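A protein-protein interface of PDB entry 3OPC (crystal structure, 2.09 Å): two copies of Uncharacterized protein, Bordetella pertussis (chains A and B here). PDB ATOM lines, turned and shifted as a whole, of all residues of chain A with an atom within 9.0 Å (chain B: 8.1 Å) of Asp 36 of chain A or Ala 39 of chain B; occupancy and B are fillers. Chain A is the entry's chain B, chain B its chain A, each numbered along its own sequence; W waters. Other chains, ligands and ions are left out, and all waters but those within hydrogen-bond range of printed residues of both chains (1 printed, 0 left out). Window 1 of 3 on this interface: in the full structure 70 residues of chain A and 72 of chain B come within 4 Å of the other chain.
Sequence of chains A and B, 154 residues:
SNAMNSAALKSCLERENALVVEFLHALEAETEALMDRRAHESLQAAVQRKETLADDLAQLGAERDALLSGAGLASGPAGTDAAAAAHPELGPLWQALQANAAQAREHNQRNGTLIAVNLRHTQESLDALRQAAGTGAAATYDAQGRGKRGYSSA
ND2 of Asn 118 of chain B is in hydrogen-bond range of O of Leu 34 of chain A.
The side-chain amide nitrogen (ND2) of Asn 118 of chain B lies close to the guanidinium group (NH1) of Arg 37 of chain A (3.3 Å).
NH2 of Arg 38 of chain B is in salt-bridge range of OD2 of Asp 36 of chain B, at 2.7 Å.
The side-chain hydroxyl (OG) of Ser 42 of chain B is in hydrogen-bond range of the backbone carbonyl oxygen (O) of Arg 38 of chain B (3.1 Å).
O of Asn 118 of chain B sits at hydrogen-bond distance from OG1 of Thr 122 of chain B, at 3.3 Å.
The guanidinium group of Arg 37 of chain A lies within hydrogen-bond range of the backbone carbonyl oxygen of Leu 34 of chain A, 2.9 Å away.
The side-chain carboxylate of Asp 36 of chain A lies within salt-bridge range of the guanidinium group of Arg 38 of chain A, at 2.8 Å.
OG of Ser 42 of chain A sits at hydrogen-bond distance from O of Arg 38 of chain A, 3.4 Å away.
Among the printed residues, merely in contact across the chains: Arg 38 of chain A with Arg 38 of chain B, His 40 of chain A with His 121 of chain B, Ala 39 of chain A with Asp 36 of chain B, Ala 33 of chain A with Leu 43 of chain B, Asp 36 of chain A with Ala 39 of chain B, Glu 30 of chain A with Ala 46 of chain B, Ala 33 of chain A with Ser 42 of chain B, Glu 30 of chain A with Leu 43 of chain B, Ala 33 of chain A with Ala 39 of chain B, Arg 37 of chain A with His 121 of chain B and Ala 29 of chain A with Ala 46 of chain B.
Asp 36 of chain A touches just one residue of chain B: Ala 39.
Printed residues of chain B within 4 Å of Arg 37 of chain A: Asn 118 (3.3 Å) and His 121 (3.7 Å).
Ala 39 of chain B touches two residues of chain A.
Of the printed residues of chain A, Leu 43 of chain B touches Glu 30 and Ala 33.
Thr 122 of chain B touches none of the printed residues of chain A.
The nearest residue of chain B that does not touch Asp 36 of chain A is Arg 38 of chain B (4.6 Å).
The nearest residue of chain A that does not touch Ala 39 of chain B is Arg 38 of chain A (5.1 Å).
Hydrophobic or aromatic side chains of chain A within 4 Å of the printed part of chain B: Ala 29, Ala 33, Ala 39 and His 40.
Of the 14 printed residues of chain B, 8 touch a printed residue of chain A.
Hydrophobic or aromatic side chains of chain B within 4 Å of the printed part of chain A: Ala 39, Leu 43, Ala 46 and His 121.
Among the printed residues, 13 pairs touch across the chains.
Asp 36 of chain A touches Ala 39 of chain B, and with the chains exchanged Ala 39 of chain A touches Asp 36 of chain B.
Arg 38 of chain B touches its own counterpart, Arg 38 of chain A.
Of the 13 pairs that touch across the chains among the printed residues, 3 have their exchanged pair printed and touching as well.
Water W1 lies within hydrogen-bond range of OD2 of Asp 36 of chain A (2.5 Å) and OG of Ser 42 of chain B (3.4 Å).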
ATOM      1  N   ALA A  29      10.764  17.436   9.351  1.00  0.00           N
ATOM      2  CA  ALA A  29       9.414  17.060   9.733  1.00  0.00           C
ATOM      3  C   ALA A  29       8.530  16.880   8.486  1.00  0.00           C
ATOM      4  O   ALA A  29       7.727  15.950   8.419  1.00  0.00           O
ATOM      5  CB  ALA A  29       8.790  18.092  10.709  1.00  0.00           C
ATOM      6  N   GLU A  30       8.668  17.771   7.507  1.00  0.00           N
ATOM      7  CA  GLU A  30       7.906  17.626   6.265  1.00  0.00           C
ATOM      8  C   GLU A  30       8.222  16.310   5.539  1.00  0.00           C
ATOM      9  O   GLU A  30       7.296  15.581   5.112  1.00  0.00           O
ATOM     10  CB  GLU A  30       8.141  18.827   5.358  1.00  0.00           C
ATOM     11  CG  GLU A  30       7.488  18.733   4.015  1.00  0.00           C
ATOM     12  CD  GLU A  30       7.792  19.945   3.117  1.00  0.00           C
ATOM     13  OE1 GLU A  30       8.893  20.576   3.231  1.00  0.00           O
ATOM     14  OE2 GLU A  30       6.905  20.252   2.294  1.00  0.00           O
ATOM     15  N   THR A  31       9.515  15.992   5.431  1.00  0.00           N
ATOM     16  CA  THR A  31       9.957  14.747   4.760  1.00  0.00           C
ATOM     17  C   THR A  31       9.371  13.535   5.524  1.00  0.00           C
ATOM     18  O   THR A  31       8.782  12.636   4.930  1.00  0.00           O
ATOM     19  CB  THR A  31      11.510  14.697   4.641  1.00  0.00           C
ATOM     20  OG1 THR A  31      11.957  15.857   3.923  1.00  0.00           O
ATOM     21  CG2 THR A  31      11.999  13.425   3.912  1.00  0.00           C
ATOM     22  N   GLU A  32       9.478  13.573   6.850  1.00  0.00           N
ATOM     23  CA  GLU A  32       8.966  12.503   7.688  1.00  0.00           C
ATOM     24  C   GLU A  32       7.478  12.270   7.458  1.00  0.00           C
ATOM     25  O   GLU A  32       7.045  11.120   7.297  1.00  0.00           O
ATOM     26  CB  GLU A  32       9.232  12.801   9.149  1.00  0.00           C
ATOM     27  CG  GLU A  32      10.638  12.433   9.557  1.00  0.00           C
ATOM     28  CD  GLU A  32      10.959  12.875  10.977  1.00  0.00           C
ATOM     29  OE1 GLU A  32      10.147  13.609  11.585  1.00  0.00           O
ATOM     30  OE2 GLU A  32      12.029  12.481  11.486  1.00  0.00           O
ATOM     31  N   ALA A  33       6.718  13.354   7.392  1.00  0.00           N
ATOM     32  CA  ALA A  33       5.289  13.260   7.111  1.00  0.00           C
ATOM     33  C   ALA A  33       5.014  12.680   5.719  1.00  0.00           C
ATOM     34  O   ALA A  33       4.116  11.853   5.568  1.00  0.00           O
ATOM     35  CB  ALA A  33       4.620  14.593   7.269  1.00  0.00           C
ATOM     36  N   LEU A  34       5.797  13.098   4.721  1.00  0.00           N
ATOM     37  CA  LEU A  34       5.602  12.645   3.342  1.00  0.00           C
ATOM     38  C   LEU A  34       5.977  11.168   3.179  1.00  0.00           C
ATOM     39  O   LEU A  34       5.487  10.511   2.301  1.00  0.00           O
ATOM     40  CB  LEU A  34       6.412  13.504   2.349  1.00  0.00           C
ATOM     41  CG  LEU A  34       5.940  14.957   2.202  1.00  0.00           C
ATOM     42  CD1 LEU A  34       6.937  15.818   1.421  1.00  0.00           C
ATOM     43  CD2 LEU A  34       4.549  14.991   1.549  1.00  0.00           C
ATOM     44  N   MET A  35       6.849  10.668   4.041  1.00  0.00           N
ATOM     45  CA  MET A  35       7.298   9.295   3.978  1.00  0.00           C
ATOM     46  C   MET A  35       6.464   8.366   4.872  1.00  0.00           C
ATOM     47  O   MET A  35       6.664   7.165   4.840  1.00  0.00           O
ATOM     48  CB  MET A  35       8.759   9.236   4.386  1.00  0.00           C
ATOM     49  CG  MET A  35       9.690   9.948   3.425  1.00  0.00           C
ATOM     50  SD  MET A  35       9.735   9.143   1.644  1.00  0.00           S
ATOM     51  CE  MET A  35       8.153   9.929   0.889  1.00  0.00           C
ATOM     52  N   ASP A  36       5.539   8.924   5.648  1.00  0.00           N
ATOM     53  CA  ASP A  36       4.715   8.162   6.585  1.00  0.00           C
ATOM     54  C   ASP A  36       3.643   7.420   5.781  1.00  0.00           C
ATOM     55  O   ASP A  36       2.653   8.022   5.359  1.00  0.00           O
ATOM     56  CB  ASP A  36       4.094   9.140   7.600  1.00  0.00           C
ATOM     57  CG  ASP A  36       3.099   8.507   8.570  1.00  0.00           C
ATOM     58  OD1 ASP A  36       2.880   7.288   8.563  1.00  0.00           O
ATOM     59  OD2 ASP A  36       2.500   9.277   9.375  1.00  0.00           O
ATOM     60  N   ARG A  37       3.859   6.117   5.593  1.00  0.00           N
ATOM     61  CA  ARG A  37       2.904   5.232   4.912  1.00  0.00           C
ATOM     62  C   ARG A  37       2.131   4.318   5.875  1.00  0.00           C
ATOM     63  O   ARG A  37       1.618   3.282   5.446  1.00  0.00           O
ATOM     64  CB  ARG A  37       3.621   4.272   3.942  1.00  0.00           C
ATOM     65  CG  ARG A  37       4.622   4.815   3.039  1.00  0.00           C
ATOM     66  CD  ARG A  37       4.088   5.816   2.042  1.00  0.00           C
ATOM     67  NE  ARG A  37       5.118   6.044   1.029  1.00  0.00           N
ATOM     68  CZ  ARG A  37       5.367   7.192   0.405  1.00  0.00           C
ATOM     69  NH1 ARG A  37       4.663   8.298   0.660  1.00  0.00           N
ATOM     70  NH2 ARG A  37       6.337   7.229  -0.500  1.00  0.00           N
ATOM     71  N   ARG A  38       2.071   4.658   7.161  1.00  0.00           N
ATOM     72  CA  ARG A  38       1.380   3.804   8.126  1.00  0.00           C
ATOM     73  C   ARG A  38      -0.066   3.570   7.725  1.00  0.00           C
ATOM     74  O   ARG A  38      -0.527   2.451   7.758  1.00  0.00           O
ATOM     75  CB  ARG A  38       1.447   4.381   9.541  1.00  0.00           C
ATOM     76  CG  ARG A  38       2.823   4.171  10.234  1.00  0.00           C
ATOM     77  CD  ARG A  38       2.977   5.010  11.538  1.00  0.00           C
ATOM     78  NE  ARG A  38       2.608   6.409  11.342  1.00  0.00           N
ATOM     79  CZ  ARG A  38       2.470   7.313  12.315  1.00  0.00           C
ATOM     80  NH1 ARG A  38       2.672   7.000  13.588  1.00  0.00           N
ATOM     81  NH2 ARG A  38       2.114   8.547  12.010  1.00  0.00           N
ATOM     82  N   ALA A  39      -0.771   4.620   7.333  1.00  0.00           N
ATOM     83  CA  ALA A  39      -2.145   4.465   6.876  1.00  0.00           C
ATOM     84  C   ALA A  39      -2.214   3.605   5.603  1.00  0.00           C
ATOM     85  O   ALA A  39      -3.138   2.792   5.458  1.00  0.00           O
ATOM     86  CB  ALA A  39      -2.786   5.801   6.635  1.00  0.00           C
ATOM     87  N   HIS A  40      -1.249   3.770   4.704  1.00  0.00           N
ATOM     88  CA  HIS A  40      -1.242   2.974   3.466  1.00  0.00           C
ATOM     89  C   HIS A  40      -1.138   1.490   3.813  1.00  0.00           C
ATOM     90  O   HIS A  40      -1.929   0.687   3.303  1.00  0.00           O
ATOM     91  CB  HIS A  40      -0.129   3.401   2.496  1.00  0.00           C
ATOM     92  CG  HIS A  40       0.234   2.354   1.461  1.00  0.00           C
ATOM     93  ND1 HIS A  40       1.325   1.510   1.599  1.00  0.00           N
ATOM     94  CD2 HIS A  40      -0.327   2.036   0.265  1.00  0.00           C
ATOM     95  CE1 HIS A  40       1.407   0.708   0.547  1.00  0.00           C
ATOM     96  NE2 HIS A  40       0.420   1.010  -0.282  1.00  0.00           N
ATOM     97  N   GLU A  41      -0.171   1.139   4.676  1.00  0.00           N
ATOM     98  CA  GLU A  41       0.075  -0.248   5.075  1.00  0.00           C
ATOM     99  C   GLU A  41      -1.109  -0.886   5.784  1.00  0.00           C
ATOM    100  O   GLU A  41      -1.416  -2.051   5.565  1.00  0.00           O
ATOM    101  CB  GLU A  41       1.244  -0.328   6.046  1.00  0.00           C
ATOM    102  CG  GLU A  41       2.612  -0.162   5.441  1.00  0.00           C
ATOM    103  CD  GLU A  41       3.675  -0.058   6.542  1.00  0.00           C
ATOM    104  OE1 GLU A  41       3.539   0.824   7.425  1.00  0.00           O
ATOM    105  OE2 GLU A  41       4.627  -0.874   6.549  1.00  0.00           O
ATOM    106  N   SER A  42      -1.738  -0.114   6.669  1.00  0.00           N
ATOM    107  CA  SER A  42      -2.948  -0.550   7.372  1.00  0.00           C
ATOM    108  C   SER A  42      -4.108  -0.841   6.424  1.00  0.00           C
ATOM    109  O   SER A  42      -4.827  -1.857   6.580  1.00  0.00           O
ATOM    110  CB  SER A  42      -3.397   0.503   8.382  1.00  0.00           C
ATOM    111  OG  SER A  42      -2.579   0.427   9.525  1.00  0.00           O
ATOM    112  N   ASP B  36      -7.508   7.928   8.591  1.00  0.00           N
ATOM    113  CA  ASP B  36      -6.263   8.227   9.312  1.00  0.00           C
ATOM    114  C   ASP B  36      -5.612   9.458   8.689  1.00  0.00           C
ATOM    115  O   ASP B  36      -5.105   9.399   7.573  1.00  0.00           O
ATOM    116  CB  ASP B  36      -5.319   7.014   9.235  1.00  0.00           C
ATOM    117  CG  ASP B  36      -3.979   7.216   9.992  1.00  0.00           C
ATOM    118  OD1 ASP B  36      -3.612   8.358  10.398  1.00  0.00           O
ATOM    119  OD2 ASP B  36      -3.251   6.203  10.135  1.00  0.00           O
ATOM    120  N   ARG B  37      -5.645  10.584   9.395  1.00  0.00           N
ATOM    121  CA  ARG B  37      -5.087  11.836   8.840  1.00  0.00           C
ATOM    122  C   ARG B  37      -3.801  12.285   9.534  1.00  0.00           C
ATOM    123  O   ARG B  37      -3.392  13.429   9.383  1.00  0.00           O
ATOM    124  CB  ARG B  37      -6.120  12.983   8.908  1.00  0.00           C
ATOM    125  CG  ARG B  37      -7.535  12.669   8.459  1.00  0.00           C
ATOM    126  CD  ARG B  37      -7.645  12.352   6.981  1.00  0.00           C
ATOM    127  NE  ARG B  37      -7.239  13.475   6.135  1.00  0.00           N
ATOM    128  CZ  ARG B  37      -6.742  13.358   4.899  1.00  0.00           C
ATOM    129  NH1 ARG B  37      -6.399  14.451   4.215  1.00  0.00           N
ATOM    130  NH2 ARG B  37      -6.564  12.163   4.346  1.00  0.00           N
ATOM    131  N   ARG B  38      -3.157  11.399  10.280  1.00  0.00           N
ATOM    132  CA  ARG B  38      -1.929  11.749  11.021  1.00  0.00           C
ATOM    133  C   ARG B  38      -0.847  12.318  10.117  1.00  0.00           C
ATOM    134  O   ARG B  38      -0.262  13.353  10.422  1.00  0.00           O
ATOM    135  CB  ARG B  38      -1.382  10.541  11.810  1.00  0.00           C
ATOM    136  CG  ARG B  38      -2.298  10.141  12.961  1.00  0.00           C
ATOM    137  CD  ARG B  38      -1.889   8.823  13.587  1.00  0.00           C
ATOM    138  NE  ARG B  38      -1.805   7.760  12.594  1.00  0.00           N
ATOM    139  CZ  ARG B  38      -1.241   6.582  12.797  1.00  0.00           C
ATOM    140  NH1 ARG B  38      -0.734   6.291  13.980  1.00  0.00           N
ATOM    141  NH2 ARG B  38      -1.188   5.683  11.826  1.00  0.00           N
ATOM    142  N   ALA B  39      -0.613  11.662   8.990  1.00  0.00           N
ATOM    143  CA  ALA B  39       0.405  12.095   8.043  1.00  0.00           C
ATOM    144  C   ALA B  39       0.037  13.452   7.457  1.00  0.00           C
ATOM    145  O   ALA B  39       0.896  14.303   7.233  1.00  0.00           O
ATOM    146  CB  ALA B  39       0.530  11.096   6.939  1.00  0.00           C
ATOM    147  N   HIS B  40      -1.252  13.639   7.216  1.00  0.00           N
ATOM    148  CA  HIS B  40      -1.740  14.880   6.671  1.00  0.00           C
ATOM    149  C   HIS B  40      -1.579  16.028   7.666  1.00  0.00           C
ATOM    150  O   HIS B  40      -1.165  17.148   7.294  1.00  0.00           O
ATOM    151  CB  HIS B  40      -3.207  14.754   6.256  1.00  0.00           C
ATOM    152  CG  HIS B  40      -3.817  16.048   5.807  1.00  0.00           C
ATOM    153  ND1 HIS B  40      -3.584  16.588   4.559  1.00  0.00           N
ATOM    154  CD2 HIS B  40      -4.655  16.910   6.443  1.00  0.00           C
ATOM    155  CE1 HIS B  40      -4.244  17.731   4.447  1.00  0.00           C
ATOM    156  NE2 HIS B  40      -4.896  17.952   5.577  1.00  0.00           N
ATOM    157  N   GLU B  41      -1.922  15.771   8.925  1.00  0.00           N
ATOM    158  CA  GLU B  41      -1.775  16.808   9.956  1.00  0.00           C
ATOM    159  C   GLU B  41      -0.301  17.138  10.210  1.00  0.00           C
ATOM    160  O   GLU B  41       0.066  18.286  10.314  1.00  0.00           O
ATOM    161  CB  GLU B  41      -2.502  16.413  11.237  1.00  0.00           C
ATOM    162  CG  GLU B  41      -4.025  16.402  11.044  1.00  0.00           C
ATOM    163  CD  GLU B  41      -4.793  15.901  12.258  1.00  0.00           C
ATOM    164  OE1 GLU B  41      -4.196  15.209  13.120  1.00  0.00           O
ATOM    165  OE2 GLU B  41      -6.008  16.190  12.339  1.00  0.00           O
ATOM    166  N   SER B  42       0.546  16.126  10.292  1.00  0.00           N
ATOM    167  CA  SER B  42       1.976  16.365  10.399  1.00  0.00           C
ATOM    168  C   SER B  42       2.481  17.256   9.264  1.00  0.00           C
ATOM    169  O   SER B  42       3.217  18.206   9.504  1.00  0.00           O
ATOM    170  CB  SER B  42       2.726  15.049  10.423  1.00  0.00           C
ATOM    171  OG  SER B  42       2.432  14.420  11.645  1.00  0.00           O
ATOM    172  N   LEU B  43       2.070  16.961   8.039  1.00  0.00           N
ATOM    173  CA  LEU B  43       2.517  17.728   6.899  1.00  0.00           C
ATOM    174  C   LEU B  43       2.027  19.161   7.027  1.00  0.00           C
ATOM    175  O   LEU B  43       2.808  20.099   6.875  1.00  0.00           O
ATOM    176  CB  LEU B  43       2.000  17.145   5.591  1.00  0.00           C
ATOM    177  CG  LEU B  43       2.325  17.995   4.359  1.00  0.00           C
ATOM    178  CD1 LEU B  43       3.833  18.050   4.178  1.00  0.00           C
ATOM    179  CD2 LEU B  43       1.612  17.390   3.170  1.00  0.00           C
ATOM    180  N   GLN B  44       0.732  19.325   7.302  1.00  0.00           N
ATOM    181  CA  GLN B  44       0.188  20.664   7.480  1.00  0.00           C
ATOM    182  C   GLN B  44       0.944  21.428   8.543  1.00  0.00           C
ATOM    183  O   GLN B  44       1.270  22.591   8.328  1.00  0.00           O
ATOM    184  CB  GLN B  44      -1.313  20.655   7.767  1.00  0.00           C
ATOM    185  CG  GLN B  44      -2.167  20.907   6.505  1.00  0.00           C
ATOM    186  CD  GLN B  44      -1.536  20.344   5.227  1.00  0.00           C
ATOM    187  OE1 GLN B  44      -1.110  21.103   4.349  1.00  0.00           O
ATOM    188  NE2 GLN B  44      -1.455  19.018   5.130  1.00  0.00           N
ATOM    189  N   ALA B  45       1.242  20.791   9.670  1.00  0.00           N
ATOM    190  CA  ALA B  45       1.908  21.500  10.754  1.00  0.00           C
ATOM    191  C   ALA B  45       3.311  21.943  10.308  1.00  0.00           C
ATOM    192  O   ALA B  45       3.722  23.068  10.575  1.00  0.00           O
ATOM    193  CB  ALA B  45       1.963  20.644  12.024  1.00  0.00           C
ATOM    194  N   ALA B  46       4.033  21.068   9.616  1.00  0.00           N
ATOM    195  CA  ALA B  46       5.384  21.408   9.162  1.00  0.00           C
ATOM    196  C   ALA B  46       5.345  22.506   8.099  1.00  0.00           C
ATOM    197  O   ALA B  46       6.143  23.426   8.154  1.00  0.00           O
ATOM    198  CB  ALA B  46       6.119  20.198   8.655  1.00  0.00           C
ATOM    199  N   ASN B 118       4.312  11.320  -3.280  1.00  0.00           N
ATOM    200  CA  ASN B 118       3.416  10.876  -2.213  1.00  0.00           C
ATOM    201  C   ASN B 118       1.996  10.841  -2.732  1.00  0.00           C
ATOM    202  O   ASN B 118       1.293   9.854  -2.569  1.00  0.00           O
ATOM    203  CB  ASN B 118       3.536  11.854  -1.016  1.00  0.00           C
ATOM    204  CG  ASN B 118       2.506  11.605   0.071  1.00  0.00           C
ATOM    205  OD1 ASN B 118       1.324  11.901  -0.102  1.00  0.00           O
ATOM    206  ND2 ASN B 118       2.954  11.070   1.202  1.00  0.00           N
ATOM    207  N   HIS B 121       1.743   7.934  -5.181  1.00  0.00           N
ATOM    208  CA  HIS B 121       1.711   6.652  -4.467  1.00  0.00           C
ATOM    209  C   HIS B 121       0.291   6.383  -3.965  1.00  0.00           C
ATOM    210  O   HIS B 121      -0.273   5.312  -4.210  1.00  0.00           O
ATOM    211  CB  HIS B 121       2.671   6.651  -3.283  1.00  0.00           C
ATOM    212  CG  HIS B 121       2.692   5.363  -2.520  1.00  0.00           C
ATOM    213  ND1 HIS B 121       3.161   4.185  -3.064  1.00  0.00           N
ATOM    214  CD2 HIS B 121       2.314   5.065  -1.250  1.00  0.00           C
ATOM    215  CE1 HIS B 121       3.072   3.216  -2.169  1.00  0.00           C
ATOM    216  NE2 HIS B 121       2.564   3.723  -1.058  1.00  0.00           N
ATOM    217  N   THR B 122      -0.268   7.367  -3.263  1.00  0.00           N
ATOM    218  CA  THR B 122      -1.629   7.308  -2.771  1.00  0.00           C
ATOM    219  C   THR B 122      -2.666   7.079  -3.887  1.00  0.00           C
ATOM    220  O   THR B 122      -3.499   6.172  -3.801  1.00  0.00           O
ATOM    221  CB  THR B 122      -1.957   8.580  -1.997  1.00  0.00           C
ATOM    222  OG1 THR B 122      -1.211   8.581  -0.776  1.00  0.00           O
ATOM    223  CG2 THR B 122      -3.419   8.656  -1.673  1.00  0.00           C
HETATM  224  O   HOH W   1       3.328  11.573  10.083  1.00  0.00           O
